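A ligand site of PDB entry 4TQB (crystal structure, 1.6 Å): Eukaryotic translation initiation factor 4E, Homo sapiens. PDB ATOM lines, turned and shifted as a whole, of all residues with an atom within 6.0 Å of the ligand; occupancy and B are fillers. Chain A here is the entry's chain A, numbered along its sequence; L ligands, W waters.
NE of Arg 131 is in salt-bridge range of O5 of the ligand. The indole nitrogen of Trp 30 lies close to a nitrogen (N1) of the ligand (3.4 Å). A nitrogen (N3) of the ligand sits at hydrogen-bond distance from the side-chain carboxylate (OE1) of Glu 77, 2.8 Å away. An oxygen (O14) of the ligand sits at hydrogen-bond distance from the backbone NH (N) of Trp 76 (2.8 Å). N of Gly 182 lies within hydrogen-bond range of O1 of the ligand (3.2 Å). The side-chain amino group of Lys 136 lies within salt-bridge range of an oxygen (O6) of the ligand (2.5 Å).
The backbone carbonyl oxygen of Lys 136 is in hydrogen-bond range of the backbone NH of Asn 129 (2.7 Å). NH1 of Arg 131 is in salt-bridge range of OD1 of Asp 64. The side-chain hydroxyl of Ser 181 is in hydrogen-bond range of the side-chain hydroxyl of Ser 183 (3.1 Å).
CA of Met 75 touches O14 of the ligand, 3.2 Å away. CB of Ser 181 touches O2 of the ligand (3.7 Å). OG of Ser 183 touches O3 of the ligand (3.8 Å). Hydrophobic or aromatic side chains within 4 Å of the ligand: Trp 30, Met 75 and Trp 76. Of the 20 residues printed, 9 come within 4 Å of the ligand. Along chain A the residues within 4 Å of the ligand span positions 30 to 183. The nearest printed residue that does not touch the ligand is Trp 140 (4.04 Å).
Water W5 lies within hydrogen-bond range of an oxygen (O1) of the ligand and the backbone NH of Gly 182. Water W1 lies within hydrogen-bond range of OD1 of Asn 129 (2.5 Å), O9 of the ligand (2.8 Å), NH1 of Arg 86 (2.9 Å) and NZ of Lys 136 (3.1 Å). Water W4 lies within hydrogen-bond range of O of Lys 180, O of Thr 177 and O12 of the ligand.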
ATOM      1  N   PHE A  22     -24.494 -15.905  18.360  1.00  0.00           N
ATOM      2  CA  PHE A  22     -23.730 -15.861  17.111  1.00  0.00           C
ATOM      3  C   PHE A  22     -22.777 -14.693  17.114  1.00  0.00           C
ATOM      4  O   PHE A  22     -23.183 -13.585  17.446  1.00  0.00           O
ATOM      5  CB  PHE A  22     -24.665 -15.741  15.909  1.00  0.00           C
ATOM      6  CG  PHE A  22     -23.948 -15.684  14.594  1.00  0.00           C
ATOM      7  CD1 PHE A  22     -23.744 -16.828  13.858  1.00  0.00           C
ATOM      8  CD2 PHE A  22     -23.490 -14.482  14.099  1.00  0.00           C
ATOM      9  CE1 PHE A  22     -23.085 -16.772  12.645  1.00  0.00           C
ATOM     10  CE2 PHE A  22     -22.834 -14.409  12.881  1.00  0.00           C
ATOM     11  CZ  PHE A  22     -22.624 -15.566  12.163  1.00  0.00           C
ATOM     12  N   ASN A  24     -20.295 -12.636  14.542  1.00  0.00           N
ATOM     13  CA  ASN A  24     -19.896 -12.463  13.135  1.00  0.00           C
ATOM     14  C   ASN A  24     -18.412 -12.731  12.916  1.00  0.00           C
ATOM     15  O   ASN A  24     -17.571 -12.291  13.695  1.00  0.00           O
ATOM     16  CB  ASN A  24     -20.229 -11.056  12.625  1.00  0.00           C
ATOM     17  CG  ASN A  24     -20.081 -10.917  11.119  1.00  0.00           C
ATOM     18  OD1 ASN A  24     -19.388 -11.711  10.475  1.00  0.00           O
ATOM     19  ND2 ASN A  24     -20.734  -9.917  10.561  1.00  0.00           N
ATOM     20  N   TRP A  30     -20.127 -19.763   8.070  1.00  0.00           N
ATOM     21  CA  TRP A  30     -21.162 -19.183   8.954  1.00  0.00           C
ATOM     22  C   TRP A  30     -21.504 -20.049  10.167  1.00  0.00           C
ATOM     23  O   TRP A  30     -21.537 -19.549  11.311  1.00  0.00           O
ATOM     24  CB  TRP A  30     -22.452 -18.945   8.144  1.00  0.00           C
ATOM     25  CG  TRP A  30     -23.533 -18.222   8.879  1.00  0.00           C
ATOM     26  CD1 TRP A  30     -23.687 -16.867   8.988  1.00  0.00           C
ATOM     27  CD2 TRP A  30     -24.626 -18.808   9.585  1.00  0.00           C
ATOM     28  NE1 TRP A  30     -24.804 -16.575   9.741  1.00  0.00           N
ATOM     29  CE2 TRP A  30     -25.402 -17.753  10.118  1.00  0.00           C
ATOM     30  CE3 TRP A  30     -25.026 -20.118   9.833  1.00  0.00           C
ATOM     31  CZ2 TRP A  30     -26.554 -17.978  10.861  1.00  0.00           C
ATOM     32  CZ3 TRP A  30     -26.164 -20.341  10.579  1.00  0.00           C
ATOM     33  CH2 TRP A  30     -26.907 -19.276  11.085  1.00  0.00           C
ATOM     34  N   GLN A  31     -21.782 -21.333   9.920  1.00  0.00           N
ATOM     35  CA  GLN A  31     -22.226 -22.246  10.971  1.00  0.00           C
ATOM     36  C   GLN A  31     -21.223 -22.327  12.127  1.00  0.00           C
ATOM     37  O   GLN A  31     -21.589 -22.647  13.260  1.00  0.00           O
ATOM     38  CB  GLN A  31     -22.442 -23.636  10.385  1.00  0.00           C
ATOM     39  CG  GLN A  31     -23.109 -24.623  11.331  1.00  0.00           C
ATOM     40  CD  GLN A  31     -23.368 -25.996  10.691  1.00  0.00           C
ATOM     41  OE1 GLN A  31     -23.554 -26.987  11.390  1.00  0.00           O
ATOM     42  NE2 GLN A  31     -23.378 -26.043   9.362  1.00  0.00           N
ATOM     43  N   ASP A  64     -25.587 -12.023  17.254  1.00  0.00           N
ATOM     44  CA  ASP A  64     -27.006 -12.342  17.224  1.00  0.00           C
ATOM     45  C   ASP A  64     -27.380 -13.152  18.438  1.00  0.00           C
ATOM     46  O   ASP A  64     -26.549 -13.866  19.015  1.00  0.00           O
ATOM     47  CB  ASP A  64     -27.428 -13.190  16.001  1.00  0.00           C
ATOM     48  CG  ASP A  64     -26.885 -12.685  14.701  1.00  0.00           C
ATOM     49  OD1 ASP A  64     -26.643 -11.462  14.547  1.00  0.00           O
ATOM     50  OD2 ASP A  64     -26.736 -13.536  13.799  1.00  0.00           O
ATOM     51  N   PRO A  74     -30.932 -22.658  14.524  1.00  0.00           N
ATOM     52  CA  PRO A  74     -31.345 -21.367  13.972  1.00  0.00           C
ATOM     53  C   PRO A  74     -30.623 -21.063  12.661  1.00  0.00           C
ATOM     54  O   PRO A  74     -29.935 -20.053  12.527  1.00  0.00           O
ATOM     55  CB  PRO A  74     -30.945 -20.382  15.078  1.00  0.00           C
ATOM     56  CG  PRO A  74     -29.767 -20.974  15.677  1.00  0.00           C
ATOM     57  CD  PRO A  74     -29.974 -22.480  15.634  1.00  0.00           C
ATOM     58  N   MET A  75     -30.815 -21.949  11.701  1.00  0.00           N
ATOM     59  CA  MET A  75     -30.166 -21.819  10.401  1.00  0.00           C
ATOM     60  C   MET A  75     -31.092 -22.369   9.319  1.00  0.00           C
ATOM     61  O   MET A  75     -31.911 -23.256   9.586  1.00  0.00           O
ATOM     62  CB  MET A  75     -28.810 -22.546  10.382  1.00  0.00           C
ATOM     63  CG  MET A  75     -28.860 -24.039  10.624  1.00  0.00           C
ATOM     64  SD  MET A  75     -27.224 -24.772  10.745  1.00  0.00           S
ATOM     65  CE  MET A  75     -26.702 -24.357  12.392  1.00  0.00           C
ATOM     66  N   TRP A  76     -30.967 -21.812   8.113  1.00  0.00           N
ATOM     67  CA  TRP A  76     -31.744 -22.236   6.951  1.00  0.00           C
ATOM     68  C   TRP A  76     -31.688 -23.745   6.707  1.00  0.00           C
ATOM     69  O   TRP A  76     -32.678 -24.342   6.247  1.00  0.00           O
ATOM     70  CB  TRP A  76     -31.222 -21.561   5.669  1.00  0.00           C
ATOM     71  CG  TRP A  76     -31.181 -20.087   5.695  1.00  0.00           C
ATOM     72  CD1 TRP A  76     -32.030 -19.230   6.360  1.00  0.00           C
ATOM     73  CD2 TRP A  76     -30.230 -19.257   5.030  1.00  0.00           C
ATOM     74  NE1 TRP A  76     -31.661 -17.937   6.133  1.00  0.00           N
ATOM     75  CE2 TRP A  76     -30.559 -17.916   5.318  1.00  0.00           C
ATOM     76  CE3 TRP A  76     -29.113 -19.522   4.215  1.00  0.00           C
ATOM     77  CZ2 TRP A  76     -29.820 -16.845   4.823  1.00  0.00           C
ATOM     78  CZ3 TRP A  76     -28.388 -18.453   3.717  1.00  0.00           C
ATOM     79  CH2 TRP A  76     -28.745 -17.136   4.021  1.00  0.00           C
ATOM     80  N   GLU A  77     -30.537 -24.341   6.987  1.00  0.00           N
ATOM     81  CA  GLU A  77     -30.249 -25.746   6.706  1.00  0.00           C
ATOM     82  C   GLU A  77     -31.141 -26.737   7.438  1.00  0.00           C
ATOM     83  O   GLU A  77     -31.338 -27.873   6.995  1.00  0.00           O
ATOM     84  CB  GLU A  77     -28.799 -26.081   7.082  1.00  0.00           C
ATOM     85  CG  GLU A  77     -27.801 -25.423   6.208  1.00  0.00           C
ATOM     86  CD  GLU A  77     -27.259 -24.126   6.755  1.00  0.00           C
ATOM     87  OE1 GLU A  77     -28.065 -23.250   7.134  1.00  0.00           O
ATOM     88  OE2 GLU A  77     -26.031 -23.981   6.762  1.00  0.00           O
ATOM     89  N   ARG A  86     -39.067 -15.832   6.929  1.00  0.00           N
ATOM     90  CA  ARG A  86     -39.123 -14.977   8.116  1.00  0.00           C
ATOM     91  C   ARG A  86     -39.845 -13.663   7.894  1.00  0.00           C
ATOM     92  O   ARG A  86     -39.749 -13.070   6.824  1.00  0.00           O
ATOM     93  CB  ARG A  86     -37.710 -14.677   8.605  1.00  0.00           C
ATOM     94  CG  ARG A  86     -36.908 -13.836   7.629  1.00  0.00           C
ATOM     95  CD  ARG A  86     -35.522 -13.495   8.106  1.00  0.00           C
ATOM     96  NE  ARG A  86     -34.763 -12.881   7.009  1.00  0.00           N
ATOM     97  CZ  ARG A  86     -33.622 -12.228   7.157  1.00  0.00           C
ATOM     98  NH1 ARG A  86     -33.065 -12.086   8.358  1.00  0.00           N
ATOM     99  NH2 ARG A  86     -33.025 -11.697   6.101  1.00  0.00           N
ATOM    100  N   ASN A 129     -30.496  -9.539  15.127  1.00  0.00           N
ATOM    101  CA  ASN A 129     -29.185  -9.170  14.617  1.00  0.00           C
ATOM    102  C   ASN A 129     -28.857  -7.752  15.063  1.00  0.00           C
ATOM    103  O   ASN A 129     -29.564  -6.793  14.731  1.00  0.00           O
ATOM    104  CB  ASN A 129     -29.107  -9.231  13.089  1.00  0.00           C
ATOM    105  CG  ASN A 129     -29.706 -10.514  12.486  1.00  0.00           C
ATOM    106  OD1 ASN A 129     -30.715 -10.452  11.790  1.00  0.00           O
ATOM    107  ND2 ASN A 129     -29.034 -11.647  12.687  1.00  0.00           N
ATOM    108  N   ARG A 131     -26.547  -4.836  14.361  1.00  0.00           N
ATOM    109  CA  ARG A 131     -25.693  -4.383  13.267  1.00  0.00           C
ATOM    110  C   ARG A 131     -25.514  -2.846  13.279  1.00  0.00           C
ATOM    111  O   ARG A 131     -26.469  -2.101  13.572  1.00  0.00           O
ATOM    112  CB  ARG A 131     -26.274  -4.831  11.931  1.00  0.00           C
ATOM    113  CG  ARG A 131     -26.477  -6.355  11.815  1.00  0.00           C
ATOM    114  CD  ARG A 131     -25.157  -7.011  11.419  1.00  0.00           C
ATOM    115  NE  ARG A 131     -25.361  -8.427  11.181  1.00  0.00           N
ATOM    116  CZ  ARG A 131     -25.444  -9.350  12.127  1.00  0.00           C
ATOM    117  NH1 ARG A 131     -25.332  -9.000  13.409  1.00  0.00           N
ATOM    118  NH2 ARG A 131     -25.651 -10.603  11.797  1.00  0.00           N
ATOM    119  N   LYS A 133     -25.434  -1.102  10.807  1.00  0.00           N
ATOM    120  CA  LYS A 133     -26.241  -0.645   9.685  1.00  0.00           C
ATOM    121  C   LYS A 133     -27.712  -0.390  10.064  1.00  0.00           C
ATOM    122  O   LYS A 133     -28.338   0.512   9.533  1.00  0.00           O
ATOM    123  CB  LYS A 133     -26.138  -1.691   8.576  1.00  0.00           C
ATOM    124  CG  LYS A 133     -26.433  -1.192   7.183  1.00  0.00           C
ATOM    125  CD  LYS A 133     -26.129  -2.269   6.131  1.00  0.00           C
ATOM    126  CE  LYS A 133     -24.642  -2.541   5.966  1.00  0.00           C
ATOM    127  NZ  LYS A 133     -24.382  -3.699   5.049  1.00  0.00           N
ATOM    128  N   LYS A 136     -31.956  -5.751  13.300  1.00  0.00           N
ATOM    129  CA  LYS A 136     -33.022  -6.538  12.741  1.00  0.00           C
ATOM    130  C   LYS A 136     -33.542  -7.546  13.741  1.00  0.00           C
ATOM    131  O   LYS A 136     -32.779  -8.184  14.470  1.00  0.00           O
ATOM    132  CB  LYS A 136     -32.543  -7.264  11.490  1.00  0.00           C
ATOM    133  CG  LYS A 136     -32.105  -6.292  10.386  1.00  0.00           C
ATOM    134  CD  LYS A 136     -31.716  -7.013   9.108  1.00  0.00           C
ATOM    135  CE  LYS A 136     -30.409  -7.721   9.236  1.00  0.00           C
ATOM    136  NZ  LYS A 136     -29.942  -8.227   7.888  1.00  0.00           N
ATOM    137  N   TRP A 140     -39.025 -16.586  12.470  1.00  0.00           N
ATOM    138  CA  TRP A 140     -38.869 -17.629  11.490  1.00  0.00           C
ATOM    139  C   TRP A 140     -40.019 -18.637  11.585  1.00  0.00           C
ATOM    140  O   TRP A 140     -40.350 -19.068  12.686  1.00  0.00           O
ATOM    141  CB  TRP A 140     -37.530 -18.345  11.718  1.00  0.00           C
ATOM    142  CG  TRP A 140     -36.290 -17.574  11.366  1.00  0.00           C
ATOM    143  CD1 TRP A 140     -36.084 -16.236  11.458  1.00  0.00           C
ATOM    144  CD2 TRP A 140     -35.085 -18.138  10.848  1.00  0.00           C
ATOM    145  NE1 TRP A 140     -34.810 -15.933  11.039  1.00  0.00           N
ATOM    146  CE2 TRP A 140     -34.170 -17.073  10.670  1.00  0.00           C
ATOM    147  CE3 TRP A 140     -34.676 -19.428  10.552  1.00  0.00           C
ATOM    148  CZ2 TRP A 140     -32.884 -17.276  10.185  1.00  0.00           C
ATOM    149  CZ3 TRP A 140     -33.396 -19.628  10.061  1.00  0.00           C
ATOM    150  CH2 TRP A 140     -32.514 -18.554   9.890  1.00  0.00           C
ATOM    151  N   THR A 177     -33.547 -15.862   0.219  1.00  0.00           N
ATOM    152  CA  THR A 177     -32.492 -15.191   0.968  1.00  0.00           C
ATOM    153  C   THR A 177     -31.160 -15.861   0.703  1.00  0.00           C
ATOM    154  O   THR A 177     -30.150 -15.181   0.545  1.00  0.00           O
ATOM    155  CB  THR A 177     -32.779 -15.188   2.490  1.00  0.00           C
ATOM    156  OG1 THR A 177     -34.097 -14.674   2.720  1.00  0.00           O
ATOM    157  CG2 THR A 177     -31.767 -14.313   3.194  1.00  0.00           C
ATOM    158  N   LYS A 180     -29.635 -14.457  -2.331  1.00  0.00           N
ATOM    159  CA  LYS A 180     -29.428 -13.001  -2.419  1.00  0.00           C
ATOM    160  C   LYS A 180     -29.016 -12.418  -1.056  1.00  0.00           C
ATOM    161  O   LYS A 180     -28.020 -12.840  -0.474  1.00  0.00           O
ATOM    162  CB  LYS A 180     -30.695 -12.316  -2.957  1.00  0.00           C
ATOM    163  CG  LYS A 180     -30.928 -12.477  -4.456  1.00  0.00           C
ATOM    164  CD  LYS A 180     -29.806 -11.869  -5.284  1.00  0.00           C
ATOM    165  CE  LYS A 180     -29.686 -10.358  -5.079  1.00  0.00           C
ATOM    166  NZ  LYS A 180     -28.620  -9.781  -5.927  1.00  0.00           N
ATOM    167  N   SER A 181     -29.783 -11.448  -0.532  1.00  0.00           N
ATOM    168  CA  SER A 181     -29.421 -10.800   0.736  1.00  0.00           C
ATOM    169  C   SER A 181     -30.665 -10.220   1.391  1.00  0.00           C
ATOM    170  O   SER A 181     -31.516  -9.647   0.715  1.00  0.00           O
ATOM    171  CB  SER A 181     -28.378  -9.700   0.509  1.00  0.00           C
ATOM    172  OG  SER A 181     -28.963  -8.530  -0.026  1.00  0.00           O
ATOM    173  N   GLY A 182     -30.777 -10.371   2.706  1.00  0.00           N
ATOM    174  CA  GLY A 182     -31.987 -10.011   3.422  1.00  0.00           C
ATOM    175  C   GLY A 182     -32.481  -8.595   3.179  1.00  0.00           C
ATOM    176  O   GLY A 182     -33.638  -8.267   3.467  1.00  0.00           O
ATOM    177  N   SER A 183     -31.590  -7.757   2.652  1.00  0.00           N
ATOM    178  CA  SER A 183     -31.934  -6.393   2.265  1.00  0.00           C
ATOM    179  C   SER A 183     -32.517  -6.349   0.858  1.00  0.00           C
ATOM    180  O   SER A 183     -33.582  -5.770   0.634  1.00  0.00           O
ATOM    181  CB  SER A 183     -30.702  -5.495   2.361  1.00  0.00           C
ATOM    182  OG  SER A 183     -29.602  -6.079   1.696  1.00  0.00           O
HETATM  183  P1  LIG L   1     -27.237  -9.103   4.826  1.00  0.00           P
HETATM  184  O1  LIG L   1     -28.539  -9.848   4.997  1.00  0.00           O
HETATM  185  O2  LIG L   1     -26.459  -9.763   3.705  1.00  0.00           O
HETATM  186  O3  LIG L   1     -27.501  -7.661   4.446  1.00  0.00           O
HETATM  187  O4  LIG L   1     -26.310  -9.180   6.133  1.00  0.00           O
HETATM  188  P2  LIG L   1     -26.772  -9.235   7.662  1.00  0.00           P
HETATM  189  O5  LIG L   1     -25.562  -9.389   8.533  1.00  0.00           O
HETATM  190  O6  LIG L   1     -27.482  -7.960   8.006  1.00  0.00           O
HETATM  191  O7  LIG L   1     -27.767 -10.471   7.844  1.00  0.00           O
HETATM  192  P3  LIG L   1     -27.343 -11.974   8.187  1.00  0.00           P
HETATM  193  O8  LIG L   1     -26.349 -11.988   9.325  1.00  0.00           O
HETATM  194  O9  LIG L   1     -28.597 -12.736   8.555  1.00  0.00           O
HETATM  195  O10 LIG L   1     -26.726 -12.730   6.934  1.00  0.00           O
HETATM  196  C1  LIG L   1     -25.415 -12.444   6.425  1.00  0.00           C
HETATM  197  C2  LIG L   1     -24.917 -13.617   5.610  1.00  0.00           C
HETATM  198  O11 LIG L   1     -24.676 -14.921   6.638  1.00  0.00           O
HETATM  199  C3  LIG L   1     -25.735 -14.003   4.748  1.00  0.00           C
HETATM  200  O12 LIG L   1     -25.527 -13.321   3.420  1.00  0.00           O
HETATM  201  C4  LIG L   1     -25.387 -15.521   4.558  1.00  0.00           C
HETATM  202  O13 LIG L   1     -24.345 -15.673   3.756  1.00  0.00           O
HETATM  203  C5  LIG L   1     -25.009 -15.994   5.988  1.00  0.00           C
HETATM  204  N1  LIG L   1     -26.147 -16.574   6.622  1.00  0.00           N
HETATM  205  C6  LIG L   1     -27.141 -15.964   7.286  1.00  0.00           C
HETATM  206  N2  LIG L   1     -27.982 -16.873   7.742  1.00  0.00           N
HETATM  207  C7  LIG L   1     -29.193 -16.597   8.505  1.00  0.00           C
HETATM  208  C8  LIG L   1     -27.547 -18.115   7.386  1.00  0.00           C
HETATM  209  C9  LIG L   1     -28.032 -19.517   7.595  1.00  0.00           C
HETATM  210  O14 LIG L   1     -29.054 -19.766   8.199  1.00  0.00           O
HETATM  211  N3  LIG L   1     -27.289 -20.584   7.059  1.00  0.00           N
HETATM  212  C10 LIG L   1     -26.079 -20.335   6.330  1.00  0.00           C
HETATM  213  N4  LIG L   1     -25.303 -21.402   5.778  1.00  0.00           N
HETATM  214  N5  LIG L   1     -25.614 -18.988   6.129  1.00  0.00           N
HETATM  215  C11 LIG L   1     -26.371 -17.896   6.676  1.00  0.00           C
HETATM  216  O   HOH W   1     -30.606 -10.964   9.295  1.00  0.00           O
HETATM  217  O   HOH W   2     -26.689  -5.350   8.034  1.00  0.00           O
HETATM  218  O   HOH W   3     -29.779 -13.483   6.397  1.00  0.00           O
HETATM  219  O   HOH W   4     -28.313 -13.895   1.819  1.00  0.00           O
HETATM  220  O   HOH W   5     -29.042 -12.067   4.022  1.00  0.00           O
